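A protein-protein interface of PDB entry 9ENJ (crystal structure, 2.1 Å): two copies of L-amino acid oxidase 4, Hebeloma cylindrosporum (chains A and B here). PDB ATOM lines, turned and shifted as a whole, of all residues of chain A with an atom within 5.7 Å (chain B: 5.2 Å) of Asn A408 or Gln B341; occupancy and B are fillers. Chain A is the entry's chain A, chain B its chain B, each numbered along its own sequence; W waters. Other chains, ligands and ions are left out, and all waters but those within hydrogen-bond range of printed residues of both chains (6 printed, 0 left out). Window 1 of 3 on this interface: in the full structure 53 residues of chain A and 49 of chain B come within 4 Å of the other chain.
The backbone NH of Phe B471 is in hydrogen-bond range of the backbone carbonyl oxygen of Gln B341 (2.8 Å).
The backbone NH (N) of Gly B473 sits at hydrogen-bond distance from the side-chain carboxylate (OD2) of Asp B476 (2.9 Å).
O of Thr A222 lies within hydrogen-bond range of OG1 of Thr A407 (2.6 Å).
The side-chain amide nitrogen (ND2) of Asn A408 lies within hydrogen-bond range of the side-chain carboxylate (OE1) of Glu A411 (3.0 Å).
N of Asn A408 sits at hydrogen-bond distance from O of Thr A222 (2.9 Å).
The side-chain carboxylate (OD2) of Asp B476 lies within hydrogen-bond range of the backbone NH (N) of Gln B341, 3.1 Å away.
Water W2 bridges OD1 of Asn A408 and NZ of Lys B339.
Water W3 lies within hydrogen-bond range of OD2 of Asp A226 (2.6 Å) and NE2 of Gln B341 (2.8 Å).
Water W4 lies within hydrogen-bond range of the backbone carbonyl oxygen of Tyr B342 (2.7 Å), the guanidinium group of Arg B227 (2.8 Å) and the side-chain carboxylate of Glu A411 (2.9 Å).
Water W1 lies within hydrogen-bond range of the side-chain carboxylate of Asp A226 and the side-chain amino group of Lys B339.
Water W6 bridges the backbone NH of Tyr B342 (3.0 Å) and the guanidinium group of Arg A412 (3.0 Å).
Water W5 lies within hydrogen-bond range of the side-chain amide oxygen of Asn A408 (3.1 Å), the backbone carbonyl oxygen of Lys B339 (3.3 Å) and the guanidinium group of Arg A412 (3.4 Å).
Among the printed residues, merely in contact across the chains: Thr A222 with Lys B339 (3.9 Å), Asp A226 with Gly B473 (3.9 Å) and Arg A412 with Tyr B342 (3.9 Å).
No position is printed for both chains.
Of the printed residues of chain B, Asp A226 touches Gly B473.
Thr A407 touches none of the printed residues of chain B.
Asn A408 touches just one residue of chain B: Gln B341 (3.1 Å).
Of the printed residues of chain B, Arg A412 touches Leu B340 (2.8 Å) and Tyr B342 (3.9 Å).
Of the printed residues of chain A, Lys B339 touches Thr A222.
Of the printed residues of chain A, Leu B340 touches Arg A412 (2.8 Å).
Gln B341 touches just one residue of chain A: Asn A408 (3.1 Å).
Printed residues of chain A within 4 Å of Tyr B342: Arg A412.
Ala B470 touches none of the printed residues of chain A.
Of the 12 printed residues of chain B, 5 touch a printed residue of chain A.
Printed residues of chain B that touch a printed residue of chain A: Lys B339, Leu B340, Gln B341, Tyr B342 and Gly B473.
Printed residues of chain A that touch a printed residue of chain B: Thr A222, Asp A226, Asn A408 and Arg A412.
Along chain A the printed residues that touch a printed residue of chain B span positions 222 to 412.
Among the printed residues, 5 pairs touch across the chains.
Among the printed residues, no Asp or Glu carboxylate lies within 4 Å of a Lys or Arg side-chain nitrogen of the other chain.
The side-chain amide oxygen (OE1) of Gln B341 is in hydrogen-bond range of the side-chain amide nitrogen (ND2) of Asn A408, at 3.1 Å.
The guanidinium group of Arg A412 lies within hydrogen-bond range of the backbone carbonyl oxygen of Leu B340 (2.8 Å).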
ATOM      1  N   SER A 221     -23.440   4.999  36.404  1.00  0.00           N
ATOM      2  CA  SER A 221     -22.162   4.923  35.708  1.00  0.00           C
ATOM      3  C   SER A 221     -22.129   5.971  34.608  1.00  0.00           C
ATOM      4  O   SER A 221     -23.158   6.530  34.220  1.00  0.00           O
ATOM      5  CB  SER A 221     -21.939   3.528  35.121  1.00  0.00           C
ATOM      6  OG  SER A 221     -23.044   3.149  34.318  1.00  0.00           O
ATOM      7  N   THR A 222     -20.926   6.228  34.098  1.00  0.00           N
ATOM      8  CA  THR A 222     -20.750   7.247  33.072  1.00  0.00           C
ATOM      9  C   THR A 222     -21.511   6.858  31.810  1.00  0.00           C
ATOM     10  O   THR A 222     -21.198   5.848  31.171  1.00  0.00           O
ATOM     11  CB  THR A 222     -19.265   7.433  32.761  1.00  0.00           C
ATOM     12  OG1 THR A 222     -18.541   7.658  33.975  1.00  0.00           O
ATOM     13  CG2 THR A 222     -19.057   8.616  31.824  1.00  0.00           C
ATOM     14  N   GLY A 223     -22.519   7.658  31.460  1.00  0.00           N
ATOM     15  CA  GLY A 223     -23.336   7.417  30.290  1.00  0.00           C
ATOM     16  C   GLY A 223     -24.648   6.715  30.566  1.00  0.00           C
ATOM     17  O   GLY A 223     -25.462   6.577  29.645  1.00  0.00           O
ATOM     18  N   ASP A 226     -27.935   8.598  29.568  1.00  0.00           N
ATOM     19  CA  ASP A 226     -28.296   8.750  28.164  1.00  0.00           C
ATOM     20  C   ASP A 226     -29.093   7.566  27.638  1.00  0.00           C
ATOM     21  O   ASP A 226     -29.562   7.609  26.494  1.00  0.00           O
ATOM     22  CB  ASP A 226     -27.041   8.958  27.313  1.00  0.00           C
ATOM     23  CG  ASP A 226     -26.541  10.395  27.357  1.00  0.00           C
ATOM     24  OD1 ASP A 226     -27.267  11.271  27.880  1.00  0.00           O
ATOM     25  OD2 ASP A 226     -25.423  10.652  26.863  1.00  0.00           O
ATOM     26  N   PRO A 344     -22.647  -2.442  27.715  1.00  0.00           N
ATOM     27  CA  PRO A 344     -21.381  -3.126  27.988  1.00  0.00           C
ATOM     28  C   PRO A 344     -21.129  -3.328  29.479  1.00  0.00           C
ATOM     29  O   PRO A 344     -21.794  -2.747  30.338  1.00  0.00           O
ATOM     30  CB  PRO A 344     -20.349  -2.158  27.396  1.00  0.00           C
ATOM     31  CG  PRO A 344     -20.952  -0.813  27.676  1.00  0.00           C
ATOM     32  CD  PRO A 344     -22.458  -0.987  27.565  1.00  0.00           C
ATOM     33  N   TRP A 406     -19.706  -0.283  34.015  1.00  0.00           N
ATOM     34  CA  TRP A 406     -20.814  -0.232  33.077  1.00  0.00           C
ATOM     35  C   TRP A 406     -20.570   0.864  32.043  1.00  0.00           C
ATOM     36  O   TRP A 406     -19.649   1.675  32.166  1.00  0.00           O
ATOM     37  CB  TRP A 406     -22.140   0.042  33.799  1.00  0.00           C
ATOM     38  CG  TRP A 406     -22.562  -1.011  34.765  1.00  0.00           C
ATOM     39  CD1 TRP A 406     -22.287  -2.344  34.705  1.00  0.00           C
ATOM     40  CD2 TRP A 406     -23.355  -0.816  35.942  1.00  0.00           C
ATOM     41  NE1 TRP A 406     -22.855  -2.993  35.774  1.00  0.00           N
ATOM     42  CE2 TRP A 406     -23.518  -2.076  36.548  1.00  0.00           C
ATOM     43  CE3 TRP A 406     -23.941   0.303  36.543  1.00  0.00           C
ATOM     44  CZ2 TRP A 406     -24.240  -2.250  37.729  1.00  0.00           C
ATOM     45  CZ3 TRP A 406     -24.660   0.130  37.713  1.00  0.00           C
ATOM     46  CH2 TRP A 406     -24.803  -1.137  38.293  1.00  0.00           C
ATOM     47  N   THR A 407     -21.430   0.873  31.019  1.00  0.00           N
ATOM     48  CA  THR A 407     -21.511   1.940  30.020  1.00  0.00           C
ATOM     49  C   THR A 407     -20.137   2.484  29.625  1.00  0.00           C
ATOM     50  O   THR A 407     -19.239   1.696  29.313  1.00  0.00           O
ATOM     51  CB  THR A 407     -22.448   3.043  30.529  1.00  0.00           C
ATOM     52  OG1 THR A 407     -22.040   3.483  31.829  1.00  0.00           O
ATOM     53  CG2 THR A 407     -23.879   2.510  30.620  1.00  0.00           C
ATOM     54  N   ASN A 408     -19.953   3.812  29.607  1.00  0.00           N
ATOM     55  CA  ASN A 408     -18.715   4.370  29.063  1.00  0.00           C
ATOM     56  C   ASN A 408     -17.488   3.850  29.807  1.00  0.00           C
ATOM     57  O   ASN A 408     -16.424   3.661  29.205  1.00  0.00           O
ATOM     58  CB  ASN A 408     -18.725   5.901  29.117  1.00  0.00           C
ATOM     59  CG  ASN A 408     -19.812   6.532  28.258  1.00  0.00           C
ATOM     60  OD1 ASN A 408     -20.293   7.620  28.574  1.00  0.00           O
ATOM     61  ND2 ASN A 408     -20.193   5.868  27.171  1.00  0.00           N
ATOM     62  N   ASP A 409     -17.607   3.642  31.120  1.00  0.00           N
ATOM     63  CA  ASP A 409     -16.466   3.165  31.893  1.00  0.00           C
ATOM     64  C   ASP A 409     -16.034   1.781  31.427  1.00  0.00           C
ATOM     65  O   ASP A 409     -14.836   1.483  31.359  1.00  0.00           O
ATOM     66  CB  ASP A 409     -16.810   3.142  33.383  1.00  0.00           C
ATOM     67  CG  ASP A 409     -17.318   4.482  33.889  1.00  0.00           C
ATOM     68  OD1 ASP A 409     -16.715   5.528  33.560  1.00  0.00           O
ATOM     69  OD2 ASP A 409     -18.329   4.485  34.621  1.00  0.00           O
ATOM     70  N   ALA A 410     -17.001   0.922  31.093  1.00  0.00           N
ATOM     71  CA  ALA A 410     -16.675  -0.414  30.604  1.00  0.00           C
ATOM     72  C   ALA A 410     -16.133  -0.362  29.181  1.00  0.00           C
ATOM     73  O   ALA A 410     -15.225  -1.125  28.828  1.00  0.00           O
ATOM     74  CB  ALA A 410     -17.910  -1.314  30.675  1.00  0.00           C
ATOM     75  N   GLU A 411     -16.679   0.526  28.348  1.00  0.00           N
ATOM     76  CA  GLU A 411     -16.189   0.653  26.978  1.00  0.00           C
ATOM     77  C   GLU A 411     -14.718   1.048  26.958  1.00  0.00           C
ATOM     78  O   GLU A 411     -13.913   0.461  26.226  1.00  0.00           O
ATOM     79  CB  GLU A 411     -17.035   1.674  26.215  1.00  0.00           C
ATOM     80  CG  GLU A 411     -18.463   1.212  26.000  1.00  0.00           C
ATOM     81  CD  GLU A 411     -19.431   2.351  25.748  1.00  0.00           C
ATOM     82  OE1 GLU A 411     -19.008   3.526  25.799  1.00  0.00           O
ATOM     83  OE2 GLU A 411     -20.622   2.066  25.508  1.00  0.00           O
ATOM     84  N   ARG A 412     -14.348   2.047  27.759  1.00  0.00           N
ATOM     85  CA  ARG A 412     -12.962   2.504  27.782  1.00  0.00           C
ATOM     86  C   ARG A 412     -12.036   1.435  28.346  1.00  0.00           C
ATOM     87  O   ARG A 412     -10.982   1.145  27.768  1.00  0.00           O
ATOM     88  CB  ARG A 412     -12.855   3.793  28.597  1.00  0.00           C
ATOM     89  CG  ARG A 412     -13.603   4.962  27.990  1.00  0.00           C
ATOM     90  CD  ARG A 412     -13.496   6.186  28.867  1.00  0.00           C
ATOM     91  NE  ARG A 412     -13.960   7.386  28.183  1.00  0.00           N
ATOM     92  CZ  ARG A 412     -13.658   8.621  28.557  1.00  0.00           C
ATOM     93  NH1 ARG A 412     -12.881   8.855  29.600  1.00  0.00           N
ATOM     94  NH2 ARG A 412     -14.133   9.644  27.854  1.00  0.00           N
ATOM     95  N   MET A 413     -12.411   0.835  29.479  1.00  0.00           N
ATOM     96  CA  MET A 413     -11.560  -0.187  30.080  1.00  0.00           C
ATOM     97  C   MET A 413     -11.379  -1.383  29.154  1.00  0.00           C
ATOM     98  O   MET A 413     -10.333  -2.041  29.189  1.00  0.00           O
ATOM     99  CB  MET A 413     -12.150  -0.637  31.419  1.00  0.00           C
ATOM    100  CG  MET A 413     -11.235  -1.552  32.224  1.00  0.00           C
ATOM    101  SD  MET A 413      -9.815  -0.683  32.921  1.00  0.00           S
ATOM    102  CE  MET A 413     -10.552   0.099  34.357  1.00  0.00           C
ATOM    103  N   ARG B 227     -27.006  10.254  20.822  1.00  0.00           N
ATOM    104  CA  ARG B 227     -25.914  11.149  21.153  1.00  0.00           C
ATOM    105  C   ARG B 227     -26.382  12.597  21.008  1.00  0.00           C
ATOM    106  O   ARG B 227     -27.539  12.873  20.687  1.00  0.00           O
ATOM    107  CB  ARG B 227     -24.708  10.852  20.266  1.00  0.00           C
ATOM    108  CG  ARG B 227     -24.360   9.372  20.208  1.00  0.00           C
ATOM    109  CD  ARG B 227     -22.960   9.115  20.685  1.00  0.00           C
ATOM    110  NE  ARG B 227     -22.685   7.692  20.848  1.00  0.00           N
ATOM    111  CZ  ARG B 227     -21.599   7.214  21.436  1.00  0.00           C
ATOM    112  NH1 ARG B 227     -20.659   8.019  21.906  1.00  0.00           N
ATOM    113  NH2 ARG B 227     -21.453   5.898  21.558  1.00  0.00           N
ATOM    114  N   LYS B 339     -16.209  12.082  31.507  1.00  0.00           N
ATOM    115  CA  LYS B 339     -17.583  12.150  31.017  1.00  0.00           C
ATOM    116  C   LYS B 339     -17.686  12.486  29.535  1.00  0.00           C
ATOM    117  O   LYS B 339     -18.604  11.994  28.870  1.00  0.00           O
ATOM    118  CB  LYS B 339     -18.377  13.183  31.828  1.00  0.00           C
ATOM    119  CG  LYS B 339     -19.800  13.441  31.324  1.00  0.00           C
ATOM    120  CD  LYS B 339     -20.658  12.184  31.351  1.00  0.00           C
ATOM    121  CE  LYS B 339     -21.999  12.400  30.662  1.00  0.00           C
ATOM    122  NZ  LYS B 339     -21.854  12.630  29.196  1.00  0.00           N
ATOM    123  N   LEU B 340     -16.796  13.322  29.004  1.00  0.00           N
ATOM    124  CA  LEU B 340     -16.849  13.662  27.586  1.00  0.00           C
ATOM    125  C   LEU B 340     -16.780  12.385  26.756  1.00  0.00           C
ATOM    126  O   LEU B 340     -15.782  11.658  26.798  1.00  0.00           O
ATOM    127  CB  LEU B 340     -15.705  14.609  27.224  1.00  0.00           C
ATOM    128  CG  LEU B 340     -15.815  16.029  27.791  1.00  0.00           C
ATOM    129  CD1 LEU B 340     -14.588  16.859  27.430  1.00  0.00           C
ATOM    130  CD2 LEU B 340     -17.081  16.718  27.300  1.00  0.00           C
ATOM    131  N   GLN B 341     -17.841  12.116  25.999  1.00  0.00           N
ATOM    132  CA  GLN B 341     -18.088  10.781  25.478  1.00  0.00           C
ATOM    133  C   GLN B 341     -17.354  10.529  24.168  1.00  0.00           C
ATOM    134  O   GLN B 341     -17.254  11.410  23.308  1.00  0.00           O
ATOM    135  CB  GLN B 341     -19.588  10.554  25.270  1.00  0.00           C
ATOM    136  CG  GLN B 341     -19.939   9.098  25.006  1.00  0.00           C
ATOM    137  CD  GLN B 341     -21.434   8.837  24.974  1.00  0.00           C
ATOM    138  OE1 GLN B 341     -21.887   7.751  25.338  1.00  0.00           O
ATOM    139  NE2 GLN B 341     -22.206   9.823  24.523  1.00  0.00           N
ATOM    140  N   TYR B 342     -16.849   9.307  24.029  1.00  0.00           N
ATOM    141  CA  TYR B 342     -16.234   8.810  22.810  1.00  0.00           C
ATOM    142  C   TYR B 342     -17.178   7.835  22.116  1.00  0.00           C
ATOM    143  O   TYR B 342     -18.113   7.302  22.721  1.00  0.00           O
ATOM    144  CB  TYR B 342     -14.898   8.124  23.117  1.00  0.00           C
ATOM    145  CG  TYR B 342     -13.718   9.073  23.119  1.00  0.00           C
ATOM    146  CD1 TYR B 342     -13.683  10.170  23.970  1.00  0.00           C
ATOM    147  CD2 TYR B 342     -12.641   8.870  22.266  1.00  0.00           C
ATOM    148  CE1 TYR B 342     -12.608  11.043  23.970  1.00  0.00           C
ATOM    149  CE2 TYR B 342     -11.560   9.733  22.259  1.00  0.00           C
ATOM    150  CZ  TYR B 342     -11.548  10.818  23.112  1.00  0.00           C
ATOM    151  OH  TYR B 342     -10.474  11.680  23.103  1.00  0.00           O
ATOM    152  N   GLY B 343     -16.928   7.618  20.827  1.00  0.00           N
ATOM    153  CA  GLY B 343     -17.728   6.715  20.034  1.00  0.00           C
ATOM    154  C   GLY B 343     -16.902   5.606  19.409  1.00  0.00           C
ATOM    155  O   GLY B 343     -15.692   5.745  19.206  1.00  0.00           O
ATOM    156  N   PHE B 469     -13.198   7.930  18.282  1.00  0.00           N
ATOM    157  CA  PHE B 469     -13.039   9.377  18.322  1.00  0.00           C
ATOM    158  C   PHE B 469     -14.084   9.926  19.281  1.00  0.00           C
ATOM    159  O   PHE B 469     -15.010   9.220  19.693  1.00  0.00           O
ATOM    160  CB  PHE B 469     -13.203  10.002  16.936  1.00  0.00           C
ATOM    161  CG  PHE B 469     -14.192   9.281  16.063  1.00  0.00           C
ATOM    162  CD1 PHE B 469     -15.530   9.223  16.414  1.00  0.00           C
ATOM    163  CD2 PHE B 469     -13.783   8.656  14.895  1.00  0.00           C
ATOM    164  CE1 PHE B 469     -16.441   8.557  15.617  1.00  0.00           C
ATOM    165  CE2 PHE B 469     -14.689   7.991  14.094  1.00  0.00           C
ATOM    166  CZ  PHE B 469     -16.023   7.941  14.456  1.00  0.00           C
ATOM    167  N   ALA B 470     -13.921  11.195  19.636  1.00  0.00           N
ATOM    168  CA  ALA B 470     -14.930  11.867  20.439  1.00  0.00           C
ATOM    169  C   ALA B 470     -16.270  11.848  19.714  1.00  0.00           C
ATOM    170  O   ALA B 470     -16.351  12.091  18.506  1.00  0.00           O
ATOM    171  CB  ALA B 470     -14.513  13.307  20.732  1.00  0.00           C
ATOM    172  N   PHE B 471     -17.329  11.544  20.466  1.00  0.00           N
ATOM    173  CA  PHE B 471     -18.702  11.569  19.960  1.00  0.00           C
ATOM    174  C   PHE B 471     -19.567  11.932  21.170  1.00  0.00           C
ATOM    175  O   PHE B 471     -20.123  11.074  21.862  1.00  0.00           O
ATOM    176  CB  PHE B 471     -19.108  10.243  19.322  1.00  0.00           C
ATOM    177  CG  PHE B 471     -20.354  10.321  18.472  1.00  0.00           C
ATOM    178  CD1 PHE B 471     -21.176  11.439  18.495  1.00  0.00           C
ATOM    179  CD2 PHE B 471     -20.703   9.260  17.655  1.00  0.00           C
ATOM    180  CE1 PHE B 471     -22.319  11.493  17.716  1.00  0.00           C
ATOM    181  CE2 PHE B 471     -21.843   9.312  16.872  1.00  0.00           C
ATOM    182  CZ  PHE B 471     -22.652  10.429  16.905  1.00  0.00           C
ATOM    183  N   PHE B 472     -19.654  13.235  21.429  1.00  0.00           N
ATOM    184  CA  PHE B 472     -20.205  13.727  22.682  1.00  0.00           C
ATOM    185  C   PHE B 472     -21.678  13.372  22.824  1.00  0.00           C
ATOM    186  O   PHE B 472     -22.436  13.373  21.851  1.00  0.00           O
ATOM    187  CB  PHE B 472     -20.039  15.246  22.773  1.00  0.00           C
ATOM    188  CG  PHE B 472     -18.638  15.699  23.101  1.00  0.00           C
ATOM    189  CD1 PHE B 472     -17.595  14.793  23.216  1.00  0.00           C
ATOM    190  CD2 PHE B 472     -18.372  17.044  23.310  1.00  0.00           C
ATOM    191  CE1 PHE B 472     -16.314  15.221  23.519  1.00  0.00           C
ATOM    192  CE2 PHE B 472     -17.094  17.477  23.614  1.00  0.00           C
ATOM    193  CZ  PHE B 472     -16.065  16.565  23.720  1.00  0.00           C
ATOM    194  N   GLY B 473     -22.079  13.073  24.055  1.00  0.00           N
ATOM    195  CA  GLY B 473     -23.477  12.963  24.387  1.00  0.00           C
ATOM    196  C   GLY B 473     -24.070  14.317  24.694  1.00  0.00           C
ATOM    197  O   GLY B 473     -23.377  15.347  24.751  1.00  0.00           O
ATOM    198  N   ASP B 476     -22.488  17.526  26.922  1.00  0.00           N
ATOM    199  CA  ASP B 476     -21.031  17.539  26.999  1.00  0.00           C
ATOM    200  C   ASP B 476     -20.463  18.880  26.540  1.00  0.00           C
ATOM    201  O   ASP B 476     -19.625  19.478  27.225  1.00  0.00           O
ATOM    202  CB  ASP B 476     -20.461  16.393  26.161  1.00  0.00           C
ATOM    203  CG  ASP B 476     -20.563  15.041  26.860  1.00  0.00           C
ATOM    204  OD1 ASP B 476     -20.881  15.006  28.070  1.00  0.00           O
ATOM    205  OD2 ASP B 476     -20.321  14.006  26.195  1.00  0.00           O
HETATM  206  O   HOH W   1     -24.206  12.884  27.806  1.00  0.00           O
HETATM  207  O   HOH W   2     -21.043   9.981  28.207  1.00  0.00           O
HETATM  208  O   HOH W   3     -25.043   9.751  24.444  1.00  0.00           O
HETATM  209  O   HOH W   4     -19.468   5.099  23.408  1.00  0.00           O
HETATM  210  O   HOH W   5     -17.447   8.957  28.491  1.00  0.00           O
HETATM  211  O   HOH W   6     -16.386   7.637  26.418  1.00  0.00           O
